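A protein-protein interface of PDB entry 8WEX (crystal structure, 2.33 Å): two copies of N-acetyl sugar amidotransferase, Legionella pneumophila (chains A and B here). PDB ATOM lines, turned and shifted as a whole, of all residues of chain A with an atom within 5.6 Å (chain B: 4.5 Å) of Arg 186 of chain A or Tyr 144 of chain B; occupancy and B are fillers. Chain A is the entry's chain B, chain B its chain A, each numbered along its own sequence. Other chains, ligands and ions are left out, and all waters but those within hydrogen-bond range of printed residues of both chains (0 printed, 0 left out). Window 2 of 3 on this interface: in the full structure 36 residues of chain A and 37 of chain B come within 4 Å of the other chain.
Of the 12 printed residues of chain B, 6 touch a printed residue of chain A. Printed residues of chain B that touch a printed residue of chain A: Tyr 144, His 173, Ala 174, Gly 175, Phe 176 and His 320. Hydrophobic or aromatic side chains of chain B within 4 Å of the printed part of chain A: Tyr 144 and His 173. Among the printed residues, no Asp or Glu carboxylate lies within 4 Å of a Lys or Arg side-chain nitrogen of the other chain.
The side-chain amide nitrogen of Asn 184 of chain A lies close to the backbone carbonyl oxygen of Gly 175 of chain B (3.2 Å). NE of Arg 189 of chain A lies within hydrogen-bond range of ND1 of His 173 of chain B, at 3.3 Å. O of His 173 of chain B lies within hydrogen-bond range of NE of Arg 186 of chain A.
Of chain B, only Tyr 144 (3.6 Å), His 173 (3.2 Å), Ala 174 (3.3 Å) and His 320 (3.8 Å) come within 4 Å of Arg 186 of chain A. Printed residues of chain A within 4 Å of Tyr 144 of chain B: Arg 186. Printed residues of chain B within 4 Å of Glu 408 of chain A: His 173. Of the printed residues of chain B, Arg 189 of chain A touches His 173. Of the printed residues of chain A, Ala 174 of chain B touches Arg 186 (3.3 Å). Printed residues of chain A within 4 Å of Phe 176 of chain B: Asn 184. Val 187 of chain A touches none of the printed residues of chain B. Leu 142 of chain B touches none of the printed residues of chain A. The nearest residue of chain B that does not touch Arg 186 of chain A is Gly 175 of chain B (4.1 Å). The nearest printed residue of chain A that does not touch Ala 174 of chain B is Asn 184 of chain A (5.3 Å).
The backbone carbonyl oxygen (O) of Ala 174 of chain B sits at hydrogen-bond distance from the side-chain hydroxyl (OH) of Tyr 144 of chain B (2.7 Å). The side-chain carboxylate of Glu 408 of chain A lies within salt-bridge range of the guanidinium group of Arg 189 of chain A, at 2.9 Å. NE of Arg 189 of chain A sits close to O of Gly 185 of chain A, at 3.4 Å. N of Val 187 of chain A is in hydrogen-bond range of OD1 of Asn 184 of chain A (3.1 Å). The side-chain carboxylate (OE2) of Glu 408 of chain A lies within salt-bridge range of the guanidinium group (NE) of Arg 186 of chain A, at 3.9 Å. The side-chain amide oxygen of Asn 184 of chain A sits at hydrogen-bond distance from the backbone NH of Arg 186 of chain A, at 2.9 Å.
No position is printed for both chains. Of the 10 pairs that touch across the chains among the printed residues, none has its exchanged pair printed and touching as well.
Among the printed residues, merely in contact across the chains: Asn 184 of chain A with Phe 176 of chain B, Gly 185 of chain A with His 173 of chain B, Arg 186 of chain A with Tyr 144 of chain B, Arg 186 of chain A with Ala 174 of chain B, Arg 186 of chain A with His 320 of chain B, Lys 407 of chain A with His 320 of chain B and Glu 408 of chain A with His 173 of chain B.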
ATOM      1  N   ASN A 184      -9.910  -9.831 -18.856  1.00  0.00           N
ATOM      2  CA  ASN A 184     -10.456 -10.423 -20.095  1.00  0.00           C
ATOM      3  C   ASN A 184     -11.774  -9.730 -20.426  1.00  0.00           C
ATOM      4  O   ASN A 184     -12.722  -9.893 -19.665  1.00  0.00           O
ATOM      5  CB  ASN A 184     -10.618 -11.933 -19.908  1.00  0.00           C
ATOM      6  CG  ASN A 184     -11.203 -12.631 -21.114  1.00  0.00           C
ATOM      7  OD1 ASN A 184     -12.066 -12.085 -21.816  1.00  0.00           O
ATOM      8  ND2 ASN A 184     -10.741 -13.846 -21.341  1.00  0.00           N
ATOM      9  N   GLY A 185     -11.822  -9.011 -21.543  1.00  0.00           N
ATOM     10  CA  GLY A 185     -12.956  -8.158 -21.937  1.00  0.00           C
ATOM     11  C   GLY A 185     -14.226  -8.956 -22.189  1.00  0.00           C
ATOM     12  O   GLY A 185     -15.310  -8.438 -21.902  1.00  0.00           O
ATOM     13  N   ARG A 186     -14.110 -10.168 -22.736  1.00  0.00           N
ATOM     14  CA  ARG A 186     -15.290 -11.036 -22.991  1.00  0.00           C
ATOM     15  C   ARG A 186     -15.861 -11.497 -21.655  1.00  0.00           C
ATOM     16  O   ARG A 186     -17.054 -11.299 -21.427  1.00  0.00           O
ATOM     17  CB  ARG A 186     -14.920 -12.245 -23.847  1.00  0.00           C
ATOM     18  CG  ARG A 186     -14.335 -11.835 -25.184  1.00  0.00           C
ATOM     19  CD  ARG A 186     -14.592 -12.891 -26.208  1.00  0.00           C
ATOM     20  NE  ARG A 186     -14.103 -12.495 -27.513  1.00  0.00           N
ATOM     21  CZ  ARG A 186     -13.729 -13.348 -28.449  1.00  0.00           C
ATOM     22  NH1 ARG A 186     -13.792 -14.654 -28.231  1.00  0.00           N
ATOM     23  NH2 ARG A 186     -13.311 -12.889 -29.607  1.00  0.00           N
ATOM     24  N   VAL A 187     -15.016 -12.038 -20.798  1.00  0.00           N
ATOM     25  CA  VAL A 187     -15.458 -12.501 -19.457  1.00  0.00           C
ATOM     26  C   VAL A 187     -16.084 -11.323 -18.708  1.00  0.00           C
ATOM     27  O   VAL A 187     -17.133 -11.494 -18.086  1.00  0.00           O
ATOM     28  CB  VAL A 187     -14.303 -13.146 -18.678  1.00  0.00           C
ATOM     29  CG1 VAL A 187     -14.704 -13.450 -17.249  1.00  0.00           C
ATOM     30  CG2 VAL A 187     -13.853 -14.412 -19.374  1.00  0.00           C
ATOM     31  N   HIS A 188     -15.473 -10.156 -18.784  1.00  0.00           N
ATOM     32  CA  HIS A 188     -15.948  -8.969 -18.038  1.00  0.00           C
ATOM     33  C   HIS A 188     -17.335  -8.592 -18.552  1.00  0.00           C
ATOM     34  O   HIS A 188     -18.215  -8.274 -17.722  1.00  0.00           O
ATOM     35  CB  HIS A 188     -14.948  -7.816 -18.154  1.00  0.00           C
ATOM     36  CG  HIS A 188     -15.027  -6.866 -17.015  1.00  0.00           C
ATOM     37  ND1 HIS A 188     -15.044  -7.297 -15.721  1.00  0.00           N
ATOM     38  CD2 HIS A 188     -15.079  -5.520 -16.972  1.00  0.00           C
ATOM     39  CE1 HIS A 188     -15.120  -6.256 -14.913  1.00  0.00           C
ATOM     40  NE2 HIS A 188     -15.150  -5.150 -15.661  1.00  0.00           N
ATOM     41  N   ARG A 189     -17.527  -8.599 -19.868  1.00  0.00           N
ATOM     42  CA  ARG A 189     -18.831  -8.198 -20.445  1.00  0.00           C
ATOM     43  C   ARG A 189     -19.890  -9.217 -20.023  1.00  0.00           C
ATOM     44  O   ARG A 189     -21.017  -8.802 -19.649  1.00  0.00           O
ATOM     45  CB  ARG A 189     -18.751  -8.076 -21.960  1.00  0.00           C
ATOM     46  CG  ARG A 189     -18.104  -6.775 -22.388  1.00  0.00           C
ATOM     47  CD  ARG A 189     -18.184  -6.623 -23.885  1.00  0.00           C
ATOM     48  NE  ARG A 189     -17.201  -7.473 -24.509  1.00  0.00           N
ATOM     49  CZ  ARG A 189     -17.340  -8.010 -25.710  1.00  0.00           C
ATOM     50  NH1 ARG A 189     -18.458  -7.810 -26.392  1.00  0.00           N
ATOM     51  NH2 ARG A 189     -16.354  -8.737 -26.205  1.00  0.00           N
ATOM     52  N   LEU A 190     -19.555 -10.503 -20.066  1.00  0.00           N
ATOM     53  CA  LEU A 190     -20.538 -11.554 -19.724  1.00  0.00           C
ATOM     54  C   LEU A 190     -20.952 -11.398 -18.260  1.00  0.00           C
ATOM     55  O   LEU A 190     -22.164 -11.398 -17.990  1.00  0.00           O
ATOM     56  CB  LEU A 190     -19.949 -12.939 -19.972  1.00  0.00           C
ATOM     57  CG  LEU A 190     -20.884 -14.070 -19.554  1.00  0.00           C
ATOM     58  CD1 LEU A 190     -22.204 -13.950 -20.303  1.00  0.00           C
ATOM     59  CD2 LEU A 190     -20.231 -15.421 -19.762  1.00  0.00           C
ATOM     60  N   LEU A 191     -19.986 -11.251 -17.357  1.00  0.00           N
ATOM     61  CA  LEU A 191     -20.267 -11.093 -15.916  1.00  0.00           C
ATOM     62  C   LEU A 191     -21.062  -9.808 -15.683  1.00  0.00           C
ATOM     63  O   LEU A 191     -21.979  -9.836 -14.830  1.00  0.00           O
ATOM     64  CB  LEU A 191     -18.960 -11.077 -15.131  1.00  0.00           C
ATOM     65  CG  LEU A 191     -18.203 -12.394 -15.125  1.00  0.00           C
ATOM     66  CD1 LEU A 191     -17.003 -12.285 -14.207  1.00  0.00           C
ATOM     67  CD2 LEU A 191     -19.086 -13.544 -14.692  1.00  0.00           C
ATOM     68  N   LYS A 407     -20.591 -14.707 -32.143  1.00  0.00           N
ATOM     69  CA  LYS A 407     -19.179 -14.656 -32.598  1.00  0.00           C
ATOM     70  C   LYS A 407     -18.245 -14.698 -31.386  1.00  0.00           C
ATOM     71  O   LYS A 407     -17.349 -15.552 -31.363  1.00  0.00           O
ATOM     72  CB  LYS A 407     -18.931 -13.409 -33.445  1.00  0.00           C
ATOM     73  CG  LYS A 407     -17.551 -13.379 -34.079  1.00  0.00           C
ATOM     74  CD  LYS A 407     -17.322 -12.186 -34.993  1.00  0.00           C
ATOM     75  CE  LYS A 407     -15.940 -12.177 -35.619  1.00  0.00           C
ATOM     76  NZ  LYS A 407     -14.861 -12.185 -34.598  1.00  0.00           N
ATOM     77  N   GLU A 408     -18.457 -13.840 -30.391  1.00  0.00           N
ATOM     78  CA  GLU A 408     -17.507 -13.721 -29.249  1.00  0.00           C
ATOM     79  C   GLU A 408     -17.854 -14.730 -28.160  1.00  0.00           C
ATOM     80  O   GLU A 408     -16.939 -15.099 -27.396  1.00  0.00           O
ATOM     81  CB  GLU A 408     -17.505 -12.297 -28.699  1.00  0.00           C
ATOM     82  CG  GLU A 408     -17.157 -11.265 -29.758  1.00  0.00           C
ATOM     83  CD  GLU A 408     -17.011  -9.855 -29.221  1.00  0.00           C
ATOM     84  OE1 GLU A 408     -18.071  -9.229 -28.924  1.00  0.00           O
ATOM     85  OE2 GLU A 408     -15.829  -9.401 -29.069  1.00  0.00           O
ATOM     86  N   PHE A 409     -19.115 -15.144 -28.076  1.00  0.00           N
ATOM     87  CA  PHE A 409     -19.618 -16.034 -27.002  1.00  0.00           C
ATOM     88  C   PHE A 409     -20.383 -17.214 -27.594  1.00  0.00           C
ATOM     89  O   PHE A 409     -21.602 -17.306 -27.455  1.00  0.00           O
ATOM     90  CB  PHE A 409     -20.506 -15.229 -26.062  1.00  0.00           C
ATOM     91  CG  PHE A 409     -19.871 -14.002 -25.476  1.00  0.00           C
ATOM     92  CD1 PHE A 409     -19.142 -14.067 -24.297  1.00  0.00           C
ATOM     93  CD2 PHE A 409     -20.025 -12.777 -26.105  1.00  0.00           C
ATOM     94  CE1 PHE A 409     -18.583 -12.918 -23.755  1.00  0.00           C
ATOM     95  CE2 PHE A 409     -19.476 -11.629 -25.555  1.00  0.00           C
ATOM     96  CZ  PHE A 409     -18.749 -11.706 -24.386  1.00  0.00           C
ATOM     97  N   HIS B 140      -3.865 -15.087 -29.405  1.00  0.00           N
ATOM     98  CA  HIS B 140      -5.144 -15.664 -29.880  1.00  0.00           C
ATOM     99  C   HIS B 140      -4.931 -17.114 -30.287  1.00  0.00           C
ATOM    100  O   HIS B 140      -5.772 -17.960 -29.904  1.00  0.00           O
ATOM    101  CB  HIS B 140      -5.734 -14.854 -31.015  1.00  0.00           C
ATOM    102  CG  HIS B 140      -7.156 -15.193 -31.268  1.00  0.00           C
ATOM    103  ND1 HIS B 140      -7.520 -16.224 -32.100  1.00  0.00           N
ATOM    104  CD2 HIS B 140      -8.293 -14.640 -30.809  1.00  0.00           C
ATOM    105  CE1 HIS B 140      -8.833 -16.293 -32.158  1.00  0.00           C
ATOM    106  NE2 HIS B 140      -9.326 -15.333 -31.372  1.00  0.00           N
ATOM    107  N   ILE B 141      -3.861 -17.395 -31.027  1.00  0.00           N
ATOM    108  CA  ILE B 141      -3.624 -18.776 -31.522  1.00  0.00           C
ATOM    109  C   ILE B 141      -3.172 -19.649 -30.345  1.00  0.00           C
ATOM    110  O   ILE B 141      -3.558 -20.819 -30.334  1.00  0.00           O
ATOM    111  CB  ILE B 141      -2.662 -18.804 -32.725  1.00  0.00           C
ATOM    112  CG1 ILE B 141      -2.923 -20.029 -33.613  1.00  0.00           C
ATOM    113  CG2 ILE B 141      -1.215 -18.716 -32.275  1.00  0.00           C
ATOM    114  CD1 ILE B 141      -4.280 -20.046 -34.284  1.00  0.00           C
ATOM    115  N   LEU B 142      -2.433 -19.115 -29.376  1.00  0.00           N
ATOM    116  CA  LEU B 142      -2.001 -19.939 -28.223  1.00  0.00           C
ATOM    117  C   LEU B 142      -3.229 -20.312 -27.385  1.00  0.00           C
ATOM    118  O   LEU B 142      -3.310 -21.465 -26.948  1.00  0.00           O
ATOM    119  CB  LEU B 142      -0.952 -19.198 -27.392  1.00  0.00           C
ATOM    120  CG  LEU B 142       0.431 -19.098 -28.034  1.00  0.00           C
ATOM    121  CD1 LEU B 142       1.287 -18.107 -27.274  1.00  0.00           C
ATOM    122  CD2 LEU B 142       1.119 -20.449 -28.086  1.00  0.00           C
ATOM    123  N   LYS B 143      -4.158 -19.393 -27.164  1.00  0.00           N
ATOM    124  CA  LYS B 143      -5.328 -19.673 -26.294  1.00  0.00           C
ATOM    125  C   LYS B 143      -6.322 -20.574 -27.038  1.00  0.00           C
ATOM    126  O   LYS B 143      -6.660 -21.643 -26.497  1.00  0.00           O
ATOM    127  CB  LYS B 143      -6.016 -18.393 -25.829  1.00  0.00           C
ATOM    128  CG  LYS B 143      -7.042 -18.602 -24.724  1.00  0.00           C
ATOM    129  CD  LYS B 143      -7.737 -17.307 -24.309  1.00  0.00           C
ATOM    130  CE  LYS B 143      -8.180 -17.281 -22.859  1.00  0.00           C
ATOM    131  NZ  LYS B 143      -7.082 -16.885 -21.939  1.00  0.00           N
ATOM    132  N   TYR B 144      -6.761 -20.169 -28.229  1.00  0.00           N
ATOM    133  CA  TYR B 144      -7.935 -20.757 -28.919  1.00  0.00           C
ATOM    134  C   TYR B 144      -7.545 -21.918 -29.838  1.00  0.00           C
ATOM    135  O   TYR B 144      -8.466 -22.612 -30.285  1.00  0.00           O
ATOM    136  CB  TYR B 144      -8.679 -19.684 -29.703  1.00  0.00           C
ATOM    137  CG  TYR B 144      -9.305 -18.644 -28.810  1.00  0.00           C
ATOM    138  CD1 TYR B 144     -10.457 -18.928 -28.092  1.00  0.00           C
ATOM    139  CD2 TYR B 144      -8.739 -17.387 -28.668  1.00  0.00           C
ATOM    140  CE1 TYR B 144     -11.044 -17.983 -27.268  1.00  0.00           C
ATOM    141  CE2 TYR B 144      -9.309 -16.440 -27.844  1.00  0.00           C
ATOM    142  CZ  TYR B 144     -10.462 -16.735 -27.138  1.00  0.00           C
ATOM    143  OH  TYR B 144     -11.014 -15.781 -26.328  1.00  0.00           O
ATOM    144  N   LYS B 145      -6.260 -22.148 -30.104  1.00  0.00           N
ATOM    145  CA  LYS B 145      -5.855 -23.295 -30.954  1.00  0.00           C
ATOM    146  C   LYS B 145      -4.971 -24.264 -30.166  1.00  0.00           C
ATOM    147  O   LYS B 145      -5.151 -25.473 -30.334  1.00  0.00           O
ATOM    148  CB  LYS B 145      -5.143 -22.844 -32.228  1.00  0.00           C
ATOM    149  CG  LYS B 145      -4.362 -23.960 -32.908  1.00  0.00           C
ATOM    150  CD  LYS B 145      -4.571 -24.086 -34.390  1.00  0.00           C
ATOM    151  CE  LYS B 145      -3.545 -25.012 -35.006  1.00  0.00           C
ATOM    152  NZ  LYS B 145      -3.627 -25.027 -36.483  1.00  0.00           N
ATOM    153  N   TYR B 146      -4.049 -23.766 -29.346  1.00  0.00           N
ATOM    154  CA  TYR B 146      -3.098 -24.623 -28.608  1.00  0.00           C
ATOM    155  C   TYR B 146      -3.520 -24.773 -27.144  1.00  0.00           C
ATOM    156  O   TYR B 146      -2.760 -25.375 -26.388  1.00  0.00           O
ATOM    157  CB  TYR B 146      -1.681 -24.093 -28.821  1.00  0.00           C
ATOM    158  CG  TYR B 146      -1.245 -24.236 -30.261  1.00  0.00           C
ATOM    159  CD1 TYR B 146      -0.871 -25.466 -30.780  1.00  0.00           C
ATOM    160  CD2 TYR B 146      -1.258 -23.156 -31.126  1.00  0.00           C
ATOM    161  CE1 TYR B 146      -0.490 -25.611 -32.106  1.00  0.00           C
ATOM    162  CE2 TYR B 146      -0.887 -23.282 -32.454  1.00  0.00           C
ATOM    163  CZ  TYR B 146      -0.519 -24.517 -32.955  1.00  0.00           C
ATOM    164  OH  TYR B 146      -0.164 -24.642 -34.268  1.00  0.00           O
ATOM    165  N   HIS B 173     -10.293  -7.567 -25.552  1.00  0.00           N
ATOM    166  CA  HIS B 173     -11.702  -7.966 -25.742  1.00  0.00           C
ATOM    167  C   HIS B 173     -11.798  -9.178 -26.678  1.00  0.00           C
ATOM    168  O   HIS B 173     -12.932  -9.618 -26.948  1.00  0.00           O
ATOM    169  CB  HIS B 173     -12.521  -6.770 -26.222  1.00  0.00           C
ATOM    170  CG  HIS B 173     -12.989  -5.927 -25.097  1.00  0.00           C
ATOM    171  ND1 HIS B 173     -14.247  -6.076 -24.567  1.00  0.00           N
ATOM    172  CD2 HIS B 173     -12.359  -4.981 -24.366  1.00  0.00           C
ATOM    173  CE1 HIS B 173     -14.385  -5.233 -23.562  1.00  0.00           C
ATOM    174  NE2 HIS B 173     -13.229  -4.556 -23.408  1.00  0.00           N
ATOM    175  N   ALA B 174     -10.675  -9.702 -27.159  1.00  0.00           N
ATOM    176  CA  ALA B 174     -10.649 -10.993 -27.875  1.00  0.00           C
ATOM    177  C   ALA B 174     -10.522 -12.128 -26.856  1.00  0.00           C
ATOM    178  O   ALA B 174     -10.620 -13.283 -27.266  1.00  0.00           O
ATOM    179  CB  ALA B 174      -9.528 -11.017 -28.858  1.00  0.00           C
ATOM    180  N   GLY B 175     -10.246 -11.802 -25.591  1.00  0.00           N
ATOM    181  CA  GLY B 175     -10.322 -12.772 -24.485  1.00  0.00           C
ATOM    182  C   GLY B 175      -9.020 -12.893 -23.739  1.00  0.00           C
ATOM    183  O   GLY B 175      -8.534 -14.029 -23.589  1.00  0.00           O
ATOM    184  N   PHE B 176      -8.478 -11.779 -23.257  1.00  0.00           N
ATOM    185  CA  PHE B 176      -7.164 -11.801 -22.574  1.00  0.00           C
ATOM    186  C   PHE B 176      -7.138 -10.802 -21.440  1.00  0.00           C
ATOM    187  O   PHE B 176      -7.500  -9.629 -21.664  1.00  0.00           O
ATOM    188  CB  PHE B 176      -6.043 -11.514 -23.561  1.00  0.00           C
ATOM    189  CG  PHE B 176      -6.018 -12.497 -24.691  1.00  0.00           C
ATOM    190  CD1 PHE B 176      -5.490 -13.764 -24.505  1.00  0.00           C
ATOM    191  CD2 PHE B 176      -6.554 -12.158 -25.921  1.00  0.00           C
ATOM    192  CE1 PHE B 176      -5.477 -14.673 -25.546  1.00  0.00           C
ATOM    193  CE2 PHE B 176      -6.540 -13.069 -26.960  1.00  0.00           C
ATOM    194  CZ  PHE B 176      -6.013 -14.328 -26.766  1.00  0.00           C
ATOM    195  N   HIS B 320     -10.673 -12.106 -36.228  1.00  0.00           N
ATOM    196  CA  HIS B 320     -10.929 -12.652 -34.870  1.00  0.00           C
ATOM    197  C   HIS B 320     -10.969 -11.554 -33.806  1.00  0.00           C
ATOM    198  O   HIS B 320     -11.329 -11.896 -32.684  1.00  0.00           O
ATOM    199  CB  HIS B 320      -9.892 -13.722 -34.509  1.00  0.00           C
ATOM    200  CG  HIS B 320      -9.904 -14.874 -35.447  1.00  0.00           C
ATOM    201  ND1 HIS B 320     -10.960 -15.760 -35.519  1.00  0.00           N
ATOM    202  CD2 HIS B 320      -9.021 -15.248 -36.399  1.00  0.00           C
ATOM    203  CE1 HIS B 320     -10.719 -16.638 -36.470  1.00  0.00           C
ATOM    204  NE2 HIS B 320      -9.540 -16.334 -37.038  1.00  0.00           N
